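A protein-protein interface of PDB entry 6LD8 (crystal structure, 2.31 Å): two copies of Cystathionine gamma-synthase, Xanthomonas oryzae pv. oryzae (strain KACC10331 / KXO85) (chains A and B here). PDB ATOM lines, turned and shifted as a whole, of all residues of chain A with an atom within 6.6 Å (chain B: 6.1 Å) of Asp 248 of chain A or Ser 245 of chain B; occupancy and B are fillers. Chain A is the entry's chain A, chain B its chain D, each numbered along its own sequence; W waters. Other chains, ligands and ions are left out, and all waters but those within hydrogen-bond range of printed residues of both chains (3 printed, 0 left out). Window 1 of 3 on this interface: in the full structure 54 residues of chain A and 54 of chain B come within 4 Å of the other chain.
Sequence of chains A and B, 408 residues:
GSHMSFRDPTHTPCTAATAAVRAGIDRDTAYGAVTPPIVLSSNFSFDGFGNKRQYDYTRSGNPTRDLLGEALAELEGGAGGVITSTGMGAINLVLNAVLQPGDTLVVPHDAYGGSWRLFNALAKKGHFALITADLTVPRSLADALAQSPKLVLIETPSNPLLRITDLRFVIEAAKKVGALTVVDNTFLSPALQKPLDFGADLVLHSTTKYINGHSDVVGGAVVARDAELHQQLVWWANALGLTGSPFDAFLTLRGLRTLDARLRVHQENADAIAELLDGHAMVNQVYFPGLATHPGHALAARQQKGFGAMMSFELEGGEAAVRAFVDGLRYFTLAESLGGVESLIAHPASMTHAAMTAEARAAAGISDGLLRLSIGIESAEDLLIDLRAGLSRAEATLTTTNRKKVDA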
ATOM      1  N   LEU A  40      14.927  31.792   2.230  1.00  0.00           N
ATOM      2  CA  LEU A  40      14.915  30.361   2.603  1.00  0.00           C
ATOM      3  C   LEU A  40      14.080  29.557   1.583  1.00  0.00           C
ATOM      4  O   LEU A  40      14.393  28.356   1.449  1.00  0.00           O
ATOM      5  CB  LEU A  40      14.340  30.186   4.012  1.00  0.00           C
ATOM      6  CG  LEU A  40      15.149  30.742   5.183  1.00  0.00           C
ATOM      7  CD1 LEU A  40      14.553  30.284   6.517  1.00  0.00           C
ATOM      8  CD2 LEU A  40      16.623  30.364   5.112  1.00  0.00           C
ATOM      9  N   LEU A  68      26.471  35.418  -2.381  1.00  0.00           N
ATOM     10  CA  LEU A  68      27.773  34.903  -1.916  1.00  0.00           C
ATOM     11  C   LEU A  68      28.597  34.445  -3.123  1.00  0.00           C
ATOM     12  O   LEU A  68      29.774  34.816  -3.183  1.00  0.00           O
ATOM     13  CB  LEU A  68      27.596  33.819  -0.878  1.00  0.00           C
ATOM     14  CG  LEU A  68      28.921  33.239  -0.459  1.00  0.00           C
ATOM     15  CD1 LEU A  68      29.825  34.304   0.203  1.00  0.00           C
ATOM     16  CD2 LEU A  68      28.702  32.073   0.460  1.00  0.00           C
ATOM     17  N   SER A  85      27.647  22.818   0.087  1.00  0.00           N
ATOM     18  CA  SER A  85      27.285  22.532   1.483  1.00  0.00           C
ATOM     19  C   SER A  85      28.558  22.407   2.306  1.00  0.00           C
ATOM     20  O   SER A  85      28.458  22.683   3.514  1.00  0.00           O
ATOM     21  CB  SER A  85      26.470  21.276   1.574  1.00  0.00           C
ATOM     22  OG  SER A  85      27.174  20.195   0.954  1.00  0.00           O
ATOM     23  N   ASN A 212      34.051  32.757   6.064  1.00  0.00           N
ATOM     24  CA  ASN A 212      33.005  32.928   7.106  1.00  0.00           C
ATOM     25  C   ASN A 212      33.610  33.526   8.390  1.00  0.00           C
ATOM     26  O   ASN A 212      33.034  34.425   8.953  1.00  0.00           O
ATOM     27  CB  ASN A 212      32.289  31.616   7.378  1.00  0.00           C
ATOM     28  CG  ASN A 212      31.249  31.807   8.451  1.00  0.00           C
ATOM     29  OD1 ASN A 212      31.402  31.305   9.580  1.00  0.00           O
ATOM     30  ND2 ASN A 212      30.285  32.656   8.136  1.00  0.00           N
ATOM     31  N   ASP A 216      30.948  28.872  12.466  1.00  0.00           N
ATOM     32  CA  ASP A 216      29.523  28.549  12.717  1.00  0.00           C
ATOM     33  C   ASP A 216      28.818  28.214  11.403  1.00  0.00           C
ATOM     34  O   ASP A 216      27.605  28.282  11.366  1.00  0.00           O
ATOM     35  CB  ASP A 216      28.840  29.676  13.495  1.00  0.00           C
ATOM     36  CG  ASP A 216      28.815  31.044  12.843  1.00  0.00           C
ATOM     37  OD1 ASP A 216      29.237  31.167  11.644  1.00  0.00           O
ATOM     38  OD2 ASP A 216      28.333  31.997  13.534  1.00  0.00           O
ATOM     39  N   VAL A 217      29.581  27.927  10.373  1.00  0.00           N
ATOM     40  CA  VAL A 217      29.111  27.488   9.033  1.00  0.00           C
ATOM     41  C   VAL A 217      30.130  26.489   8.486  1.00  0.00           C
ATOM     42  O   VAL A 217      31.335  26.750   8.536  1.00  0.00           O
ATOM     43  CB  VAL A 217      28.983  28.634   8.022  1.00  0.00           C
ATOM     44  CG1 VAL A 217      28.566  28.071   6.676  1.00  0.00           C
ATOM     45  CG2 VAL A 217      28.013  29.729   8.478  1.00  0.00           C
ATOM     46  N   VAL A 218      29.665  25.385   7.934  1.00  0.00           N
ATOM     47  CA  VAL A 218      30.487  24.581   7.013  1.00  0.00           C
ATOM     48  C   VAL A 218      29.947  24.890   5.621  1.00  0.00           C
ATOM     49  O   VAL A 218      28.716  24.907   5.461  1.00  0.00           O
ATOM     50  CB  VAL A 218      30.418  23.102   7.399  1.00  0.00           C
ATOM     51  CG1 VAL A 218      31.319  22.281   6.504  1.00  0.00           C
ATOM     52  CG2 VAL A 218      30.797  22.881   8.851  1.00  0.00           C
ATOM     53  N   GLY A 219      30.852  25.169   4.681  1.00  0.00           N
ATOM     54  CA  GLY A 219      30.520  25.571   3.304  1.00  0.00           C
ATOM     55  C   GLY A 219      31.731  25.512   2.373  1.00  0.00           C
ATOM     56  O   GLY A 219      32.867  25.475   2.872  1.00  0.00           O
ATOM     57  N   GLY A 244      24.479  24.550  -1.329  1.00  0.00           N
ATOM     58  CA  GLY A 244      24.362  24.949   0.085  1.00  0.00           C
ATOM     59  C   GLY A 244      23.016  25.582   0.436  1.00  0.00           C
ATOM     60  O   GLY A 244      22.270  26.091  -0.414  1.00  0.00           O
ATOM     61  N   SER A 245      22.805  25.606   1.720  1.00  0.00           N
ATOM     62  CA  SER A 245      21.671  26.233   2.435  1.00  0.00           C
ATOM     63  C   SER A 245      21.748  27.751   2.322  1.00  0.00           C
ATOM     64  O   SER A 245      22.767  28.361   2.600  1.00  0.00           O
ATOM     65  CB  SER A 245      21.746  25.742   3.830  1.00  0.00           C
ATOM     66  OG  SER A 245      21.439  26.742   4.731  1.00  0.00           O
ATOM     67  N   PRO A 246      20.660  28.391   1.874  1.00  0.00           N
ATOM     68  CA  PRO A 246      20.532  29.839   1.899  1.00  0.00           C
ATOM     69  C   PRO A 246      20.869  30.470   3.254  1.00  0.00           C
ATOM     70  O   PRO A 246      21.469  31.545   3.275  1.00  0.00           O
ATOM     71  CB  PRO A 246      19.058  30.033   1.541  1.00  0.00           C
ATOM     72  CG  PRO A 246      18.794  28.878   0.610  1.00  0.00           C
ATOM     73  CD  PRO A 246      19.457  27.738   1.343  1.00  0.00           C
ATOM     74  N   PHE A 247      20.501  29.844   4.364  1.00  0.00           N
ATOM     75  CA  PHE A 247      20.820  30.437   5.681  1.00  0.00           C
ATOM     76  C   PHE A 247      22.351  30.492   5.882  1.00  0.00           C
ATOM     77  O   PHE A 247      22.865  31.501   6.376  1.00  0.00           O
ATOM     78  CB  PHE A 247      20.138  29.668   6.800  1.00  0.00           C
ATOM     79  CG  PHE A 247      20.462  30.185   8.164  1.00  0.00           C
ATOM     80  CD1 PHE A 247      19.799  31.287   8.675  1.00  0.00           C
ATOM     81  CD2 PHE A 247      21.502  29.637   8.885  1.00  0.00           C
ATOM     82  CE1 PHE A 247      20.139  31.777   9.929  1.00  0.00           C
ATOM     83  CE2 PHE A 247      21.825  30.123  10.147  1.00  0.00           C
ATOM     84  CZ  PHE A 247      21.138  31.197  10.666  1.00  0.00           C
ATOM     85  N   ASP A 248      23.051  29.403   5.598  1.00  0.00           N
ATOM     86  CA  ASP A 248      24.527  29.325   5.694  1.00  0.00           C
ATOM     87  C   ASP A 248      25.170  30.384   4.781  1.00  0.00           C
ATOM     88  O   ASP A 248      26.194  31.013   5.174  1.00  0.00           O
ATOM     89  CB  ASP A 248      25.020  27.932   5.342  1.00  0.00           C
ATOM     90  CG  ASP A 248      24.812  26.941   6.473  1.00  0.00           C
ATOM     91  OD1 ASP A 248      24.098  27.342   7.430  1.00  0.00           O
ATOM     92  OD2 ASP A 248      25.430  25.795   6.416  1.00  0.00           O
ATOM     93  N   ALA A 249      24.572  30.647   3.637  1.00  0.00           N
ATOM     94  CA  ALA A 249      25.146  31.644   2.729  1.00  0.00           C
ATOM     95  C   ALA A 249      24.942  33.056   3.310  1.00  0.00           C
ATOM     96  O   ALA A 249      25.777  33.913   3.107  1.00  0.00           O
ATOM     97  CB  ALA A 249      24.518  31.499   1.391  1.00  0.00           C
ATOM     98  N   PHE A 250      23.821  33.305   3.956  1.00  0.00           N
ATOM     99  CA  PHE A 250      23.567  34.534   4.720  1.00  0.00           C
ATOM    100  C   PHE A 250      24.695  34.722   5.750  1.00  0.00           C
ATOM    101  O   PHE A 250      25.209  35.817   5.860  1.00  0.00           O
ATOM    102  CB  PHE A 250      22.213  34.461   5.431  1.00  0.00           C
ATOM    103  CG  PHE A 250      22.067  35.478   6.512  1.00  0.00           C
ATOM    104  CD1 PHE A 250      21.943  36.814   6.192  1.00  0.00           C
ATOM    105  CD2 PHE A 250      22.168  35.113   7.827  1.00  0.00           C
ATOM    106  CE1 PHE A 250      21.855  37.762   7.189  1.00  0.00           C
ATOM    107  CE2 PHE A 250      22.084  36.074   8.824  1.00  0.00           C
ATOM    108  CZ  PHE A 250      21.992  37.399   8.501  1.00  0.00           C
ATOM    109  N   LEU A 251      24.989  33.725   6.566  1.00  0.00           N
ATOM    110  CA  LEU A 251      25.967  33.896   7.658  1.00  0.00           C
ATOM    111  C   LEU A 251      27.370  34.088   7.066  1.00  0.00           C
ATOM    112  O   LEU A 251      28.157  34.861   7.628  1.00  0.00           O
ATOM    113  CB  LEU A 251      25.940  32.670   8.558  1.00  0.00           C
ATOM    114  CG  LEU A 251      24.921  32.672   9.683  1.00  0.00           C
ATOM    115  CD1 LEU A 251      25.158  31.455  10.547  1.00  0.00           C
ATOM    116  CD2 LEU A 251      25.013  33.955  10.529  1.00  0.00           C
ATOM    117  N   THR A 252      27.660  33.382   5.983  1.00  0.00           N
ATOM    118  CA  THR A 252      28.949  33.419   5.255  1.00  0.00           C
ATOM    119  C   THR A 252      29.128  34.810   4.644  1.00  0.00           C
ATOM    120  O   THR A 252      30.168  35.442   4.874  1.00  0.00           O
ATOM    121  CB  THR A 252      29.110  32.275   4.252  1.00  0.00           C
ATOM    122  OG1 THR A 252      28.911  31.082   5.021  1.00  0.00           O
ATOM    123  CG2 THR A 252      30.490  32.266   3.617  1.00  0.00           C
ATOM    124  N   LEU A 253      28.120  35.321   3.995  1.00  0.00           N
ATOM    125  CA  LEU A 253      28.196  36.687   3.472  1.00  0.00           C
ATOM    126  C   LEU A 253      28.424  37.697   4.626  1.00  0.00           C
ATOM    127  O   LEU A 253      29.200  38.668   4.470  1.00  0.00           O
ATOM    128  CB  LEU A 253      26.916  36.935   2.707  1.00  0.00           C
ATOM    129  CG  LEU A 253      27.006  38.132   1.766  1.00  0.00           C
ATOM    130  CD1 LEU A 253      27.847  37.846   0.534  1.00  0.00           C
ATOM    131  CD2 LEU A 253      25.639  38.558   1.333  1.00  0.00           C
ATOM    132  N   LEU B  40      25.257  25.338  15.644  1.00  0.00           N
ATOM    133  CA  LEU B  40      25.825  25.784  14.357  1.00  0.00           C
ATOM    134  C   LEU B  40      27.341  25.461  14.304  1.00  0.00           C
ATOM    135  O   LEU B  40      27.847  25.318  13.145  1.00  0.00           O
ATOM    136  CB  LEU B  40      25.577  27.278  14.179  1.00  0.00           C
ATOM    137  CG  LEU B  40      24.139  27.748  14.000  1.00  0.00           C
ATOM    138  CD1 LEU B  40      24.127  29.214  13.613  1.00  0.00           C
ATOM    139  CD2 LEU B  40      23.369  26.945  12.972  1.00  0.00           C
ATOM    140  N   ARG B  65      21.911  17.908  13.603  1.00  0.00           N
ATOM    141  CA  ARG B  65      21.654  17.089  12.404  1.00  0.00           C
ATOM    142  C   ARG B  65      21.279  15.657  12.868  1.00  0.00           C
ATOM    143  O   ARG B  65      20.355  15.068  12.307  1.00  0.00           O
ATOM    144  CB  ARG B  65      22.847  17.131  11.455  1.00  0.00           C
ATOM    145  CG  ARG B  65      22.489  16.755  10.030  1.00  0.00           C
ATOM    146  CD  ARG B  65      23.501  17.231   9.004  1.00  0.00           C
ATOM    147  NE  ARG B  65      24.677  16.465   9.256  1.00  0.00           N
ATOM    148  CZ  ARG B  65      25.904  16.942   9.427  1.00  0.00           C
ATOM    149  NH1 ARG B  65      26.235  18.212   9.214  1.00  0.00           N
ATOM    150  NH2 ARG B  65      26.824  16.072   9.768  1.00  0.00           N
ATOM    151  N   THR B  84      21.462  14.952   4.304  1.00  0.00           N
ATOM    152  CA  THR B  84      22.192  15.569   3.206  1.00  0.00           C
ATOM    153  C   THR B  84      21.667  16.973   2.940  1.00  0.00           C
ATOM    154  O   THR B  84      20.597  17.330   3.432  1.00  0.00           O
ATOM    155  CB  THR B  84      22.066  14.698   1.951  1.00  0.00           C
ATOM    156  OG1 THR B  84      20.679  14.548   1.589  1.00  0.00           O
ATOM    157  CG2 THR B  84      22.745  13.368   2.188  1.00  0.00           C
ATOM    158  N   SER B  85      22.431  17.720   2.164  1.00  0.00           N
ATOM    159  CA  SER B  85      22.151  19.118   1.753  1.00  0.00           C
ATOM    160  C   SER B  85      20.869  19.138   0.920  1.00  0.00           C
ATOM    161  O   SER B  85      20.166  20.140   0.983  1.00  0.00           O
ATOM    162  CB  SER B  85      23.301  19.662   0.927  1.00  0.00           C
ATOM    163  OG  SER B  85      23.762  18.622   0.020  1.00  0.00           O
ATOM    164  N   THR B 243      26.856  16.253   3.572  1.00  0.00           N
ATOM    165  CA  THR B 243      26.063  16.504   4.804  1.00  0.00           C
ATOM    166  C   THR B 243      25.428  17.906   4.766  1.00  0.00           C
ATOM    167  O   THR B 243      25.900  18.792   4.062  1.00  0.00           O
ATOM    168  CB  THR B 243      26.885  16.251   6.067  1.00  0.00           C
ATOM    169  OG1 THR B 243      28.104  16.989   5.941  1.00  0.00           O
ATOM    170  CG2 THR B 243      27.167  14.780   6.270  1.00  0.00           C
ATOM    171  N   GLY B 244      24.320  18.039   5.483  1.00  0.00           N
ATOM    172  CA  GLY B 244      23.492  19.255   5.558  1.00  0.00           C
ATOM    173  C   GLY B 244      23.872  20.178   6.704  1.00  0.00           C
ATOM    174  O   GLY B 244      24.534  19.783   7.678  1.00  0.00           O
ATOM    175  N   SER B 245      23.323  21.356   6.599  1.00  0.00           N
ATOM    176  CA  SER B 245      23.451  22.474   7.551  1.00  0.00           C
ATOM    177  C   SER B 245      22.675  22.176   8.832  1.00  0.00           C
ATOM    178  O   SER B 245      21.530  21.802   8.817  1.00  0.00           O
ATOM    179  CB  SER B 245      22.963  23.701   6.856  1.00  0.00           C
ATOM    180  OG  SER B 245      22.304  24.545   7.744  1.00  0.00           O
ATOM    181  N   PRO B 246      23.301  22.345   9.994  1.00  0.00           N
ATOM    182  CA  PRO B 246      22.601  22.269  11.262  1.00  0.00           C
ATOM    183  C   PRO B 246      21.349  23.157  11.335  1.00  0.00           C
ATOM    184  O   PRO B 246      20.357  22.735  11.932  1.00  0.00           O
ATOM    185  CB  PRO B 246      23.676  22.714  12.245  1.00  0.00           C
ATOM    186  CG  PRO B 246      24.960  22.236  11.588  1.00  0.00           C
ATOM    187  CD  PRO B 246      24.748  22.548  10.136  1.00  0.00           C
ATOM    188  N   PHE B 247      21.363  24.336  10.749  1.00  0.00           N
ATOM    189  CA  PHE B 247      20.182  25.207  10.839  1.00  0.00           C
ATOM    190  C   PHE B 247      18.997  24.588  10.077  1.00  0.00           C
ATOM    191  O   PHE B 247      17.847  24.670  10.530  1.00  0.00           O
ATOM    192  CB  PHE B 247      20.492  26.581  10.280  1.00  0.00           C
ATOM    193  CG  PHE B 247      19.325  27.507  10.314  1.00  0.00           C
ATOM    194  CD1 PHE B 247      18.973  28.141  11.480  1.00  0.00           C
ATOM    195  CD2 PHE B 247      18.514  27.650   9.213  1.00  0.00           C
ATOM    196  CE1 PHE B 247      17.878  28.987  11.493  1.00  0.00           C
ATOM    197  CE2 PHE B 247      17.408  28.494   9.237  1.00  0.00           C
ATOM    198  CZ  PHE B 247      17.119  29.194  10.368  1.00  0.00           C
ATOM    199  N   ASP B 248      19.245  24.118   8.872  1.00  0.00           N
ATOM    200  CA  ASP B 248      18.253  23.403   8.041  1.00  0.00           C
ATOM    201  C   ASP B 248      17.736  22.177   8.808  1.00  0.00           C
ATOM    202  O   ASP B 248      16.508  21.895   8.740  1.00  0.00           O
ATOM    203  CB  ASP B 248      18.841  23.002   6.699  1.00  0.00           C
ATOM    204  CG  ASP B 248      18.934  24.181   5.748  1.00  0.00           C
ATOM    205  OD1 ASP B 248      18.720  25.316   6.253  1.00  0.00           O
ATOM    206  OD2 ASP B 248      19.173  23.942   4.488  1.00  0.00           O
ATOM    207  N   ALA B 249      18.603  21.473   9.512  1.00  0.00           N
ATOM    208  CA  ALA B 249      18.140  20.292  10.256  1.00  0.00           C
ATOM    209  C   ALA B 249      17.197  20.725  11.391  1.00  0.00           C
ATOM    210  O   ALA B 249      16.333  19.985  11.780  1.00  0.00           O
ATOM    211  CB  ALA B 249      19.304  19.546  10.781  1.00  0.00           C
ATOM    212  N   PHE B 250      17.434  21.883  11.966  1.00  0.00           N
ATOM    213  CA  PHE B 250      16.617  22.445  13.041  1.00  0.00           C
ATOM    214  C   PHE B 250      15.216  22.749  12.476  1.00  0.00           C
ATOM    215  O   PHE B 250      14.256  22.428  13.148  1.00  0.00           O
ATOM    216  CB  PHE B 250      17.289  23.694  13.609  1.00  0.00           C
ATOM    217  CG  PHE B 250      16.316  24.609  14.276  1.00  0.00           C
ATOM    218  CD1 PHE B 250      15.837  24.309  15.543  1.00  0.00           C
ATOM    219  CD2 PHE B 250      15.816  25.709  13.610  1.00  0.00           C
ATOM    220  CE1 PHE B 250      14.889  25.122  16.138  1.00  0.00           C
ATOM    221  CE2 PHE B 250      14.861  26.516  14.221  1.00  0.00           C
ATOM    222  CZ  PHE B 250      14.381  26.199  15.462  1.00  0.00           C
HETATM  223  O   HOH W   1      23.766  25.756   9.543  1.00  0.00           O
HETATM  224  O   HOH W   2      18.856  27.350   4.669  1.00  0.00           O
HETATM  225  O   HOH W   3      26.423  25.694  10.728  1.00  0.00           O
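Ser 85 of chain B touches its own counterpart, Ser 85 of chain A.
Ser 245 of chain A touches its own counterpart, Ser 245 of chain B.
Ser 245 of chain A touches Asp 248 of chain B, and with the chains exchanged Asp 248 of chain A touches Ser 245 of chain B.
Phe 247 of chain A touches its own counterpart, Phe 247 of chain B.
Printed residues of chain B within 4 Å of Ser 245 of chain A: Ser 245 and Asp 248.
Of the printed residues of chain A, Ser 85 of chain B touches Ser 85 (3.6 Å).
Of the printed residues of chain A, Thr 243 of chain B touches Ser 85.
Ser 245 of chain B touches just these residues of chain A: Ser 245 (3.8 Å) and Asp 248 (3.3 Å).
Printed residues of chain A within 4 Å of Phe 247 of chain B: Phe 247 (3.4 Å).
The nearest residue of chain B that does not touch Asp 248 of chain A is Phe 247 of chain B (4.7 Å).
The nearest residue of chain A that does not touch Ser 245 of chain B is Phe 247 of chain A (5.3 Å).
Water W2 lies within hydrogen-bond range of OD1 of Asp 248 of chain B (2.6 Å), OG of Ser 245 of chain A (2.7 Å) and N of Phe 247 of chain A (3.0 Å).
Water W1 lies within hydrogen-bond range of OG of Ser 245 of chain B (2.6 Å), OD1 of Asp 248 of chain A (2.7 Å) and N of Phe 247 of chain B (3.0 Å).
Water W3 lies within hydrogen-bond range of O of Leu 40 of chain B and O of Asp 216 of chain A.
Among the printed residues, merely in contact across the chains: Phe 247 of chain A with Phe 247 of chain B (3.4 Å), Ser 85 of chain A with Thr 243 of chain B (3.6 Å), Ser 85 of chain A with Ser 85 of chain B (3.6 Å), Ser 245 of chain A with Ser 245 of chain B (3.8 Å) and Leu 251 of chain A with Leu 40 of chain B (3.9 Å).
OG of Ser 245 of chain A sits at hydrogen-bond distance from OD1 of Asp 248 of chain B (3.4 Å).
OG of Ser 245 of chain B sits at hydrogen-bond distance from OD1 of Asp 248 of chain A (3.3 Å).
The backbone carbonyl oxygen (O) of Asp 216 of chain A sits close to the backbone carbonyl oxygen (O) of Leu 40 of chain B (3.5 Å).
Of the 18 printed residues of chain A, 6 touch a printed residue of chain B.
Printed residues of chain B that touch a printed residue of chain A: Leu 40, Ser 85, Thr 243, Ser 245, Phe 247 and Asp 248.
Hydrophobic or aromatic side chains of chain B that line the printed part of chain A: Leu 40 and Phe 247.
Among the printed residues, no Asp or Glu carboxylate lies within 4 Å of a Lys or Arg side-chain nitrogen of the other chain.
The backbone carbonyl oxygen (O) of Leu 251 of chain A lies within hydrogen-bond range of the side-chain amide nitrogen (ND2) of Asn 212 of chain A, at 3.1 Å.
The backbone NH of Phe 247 of chain A sits close to the side-chain hydroxyl of Ser 245 of chain A (3.3 Å).
The backbone NH of Asp 248 of chain A is in hydrogen-bond range of the side-chain hydroxyl of Ser 245 of chain A (3.2 Å).
The backbone carbonyl oxygen of Asp 248 of chain A is in hydrogen-bond range of the side-chain hydroxyl of Thr 252 of chain A, 2.7 Å away.
The backbone NH (N) of Phe 247 of chain B is in hydrogen-bond range of the side-chain hydroxyl (OG) of Ser 245 of chain B.
The side-chain hydroxyl of Ser 245 of chain B sits at hydrogen-bond distance from the backbone NH of Asp 248 of chain B, at 3.3 Å.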
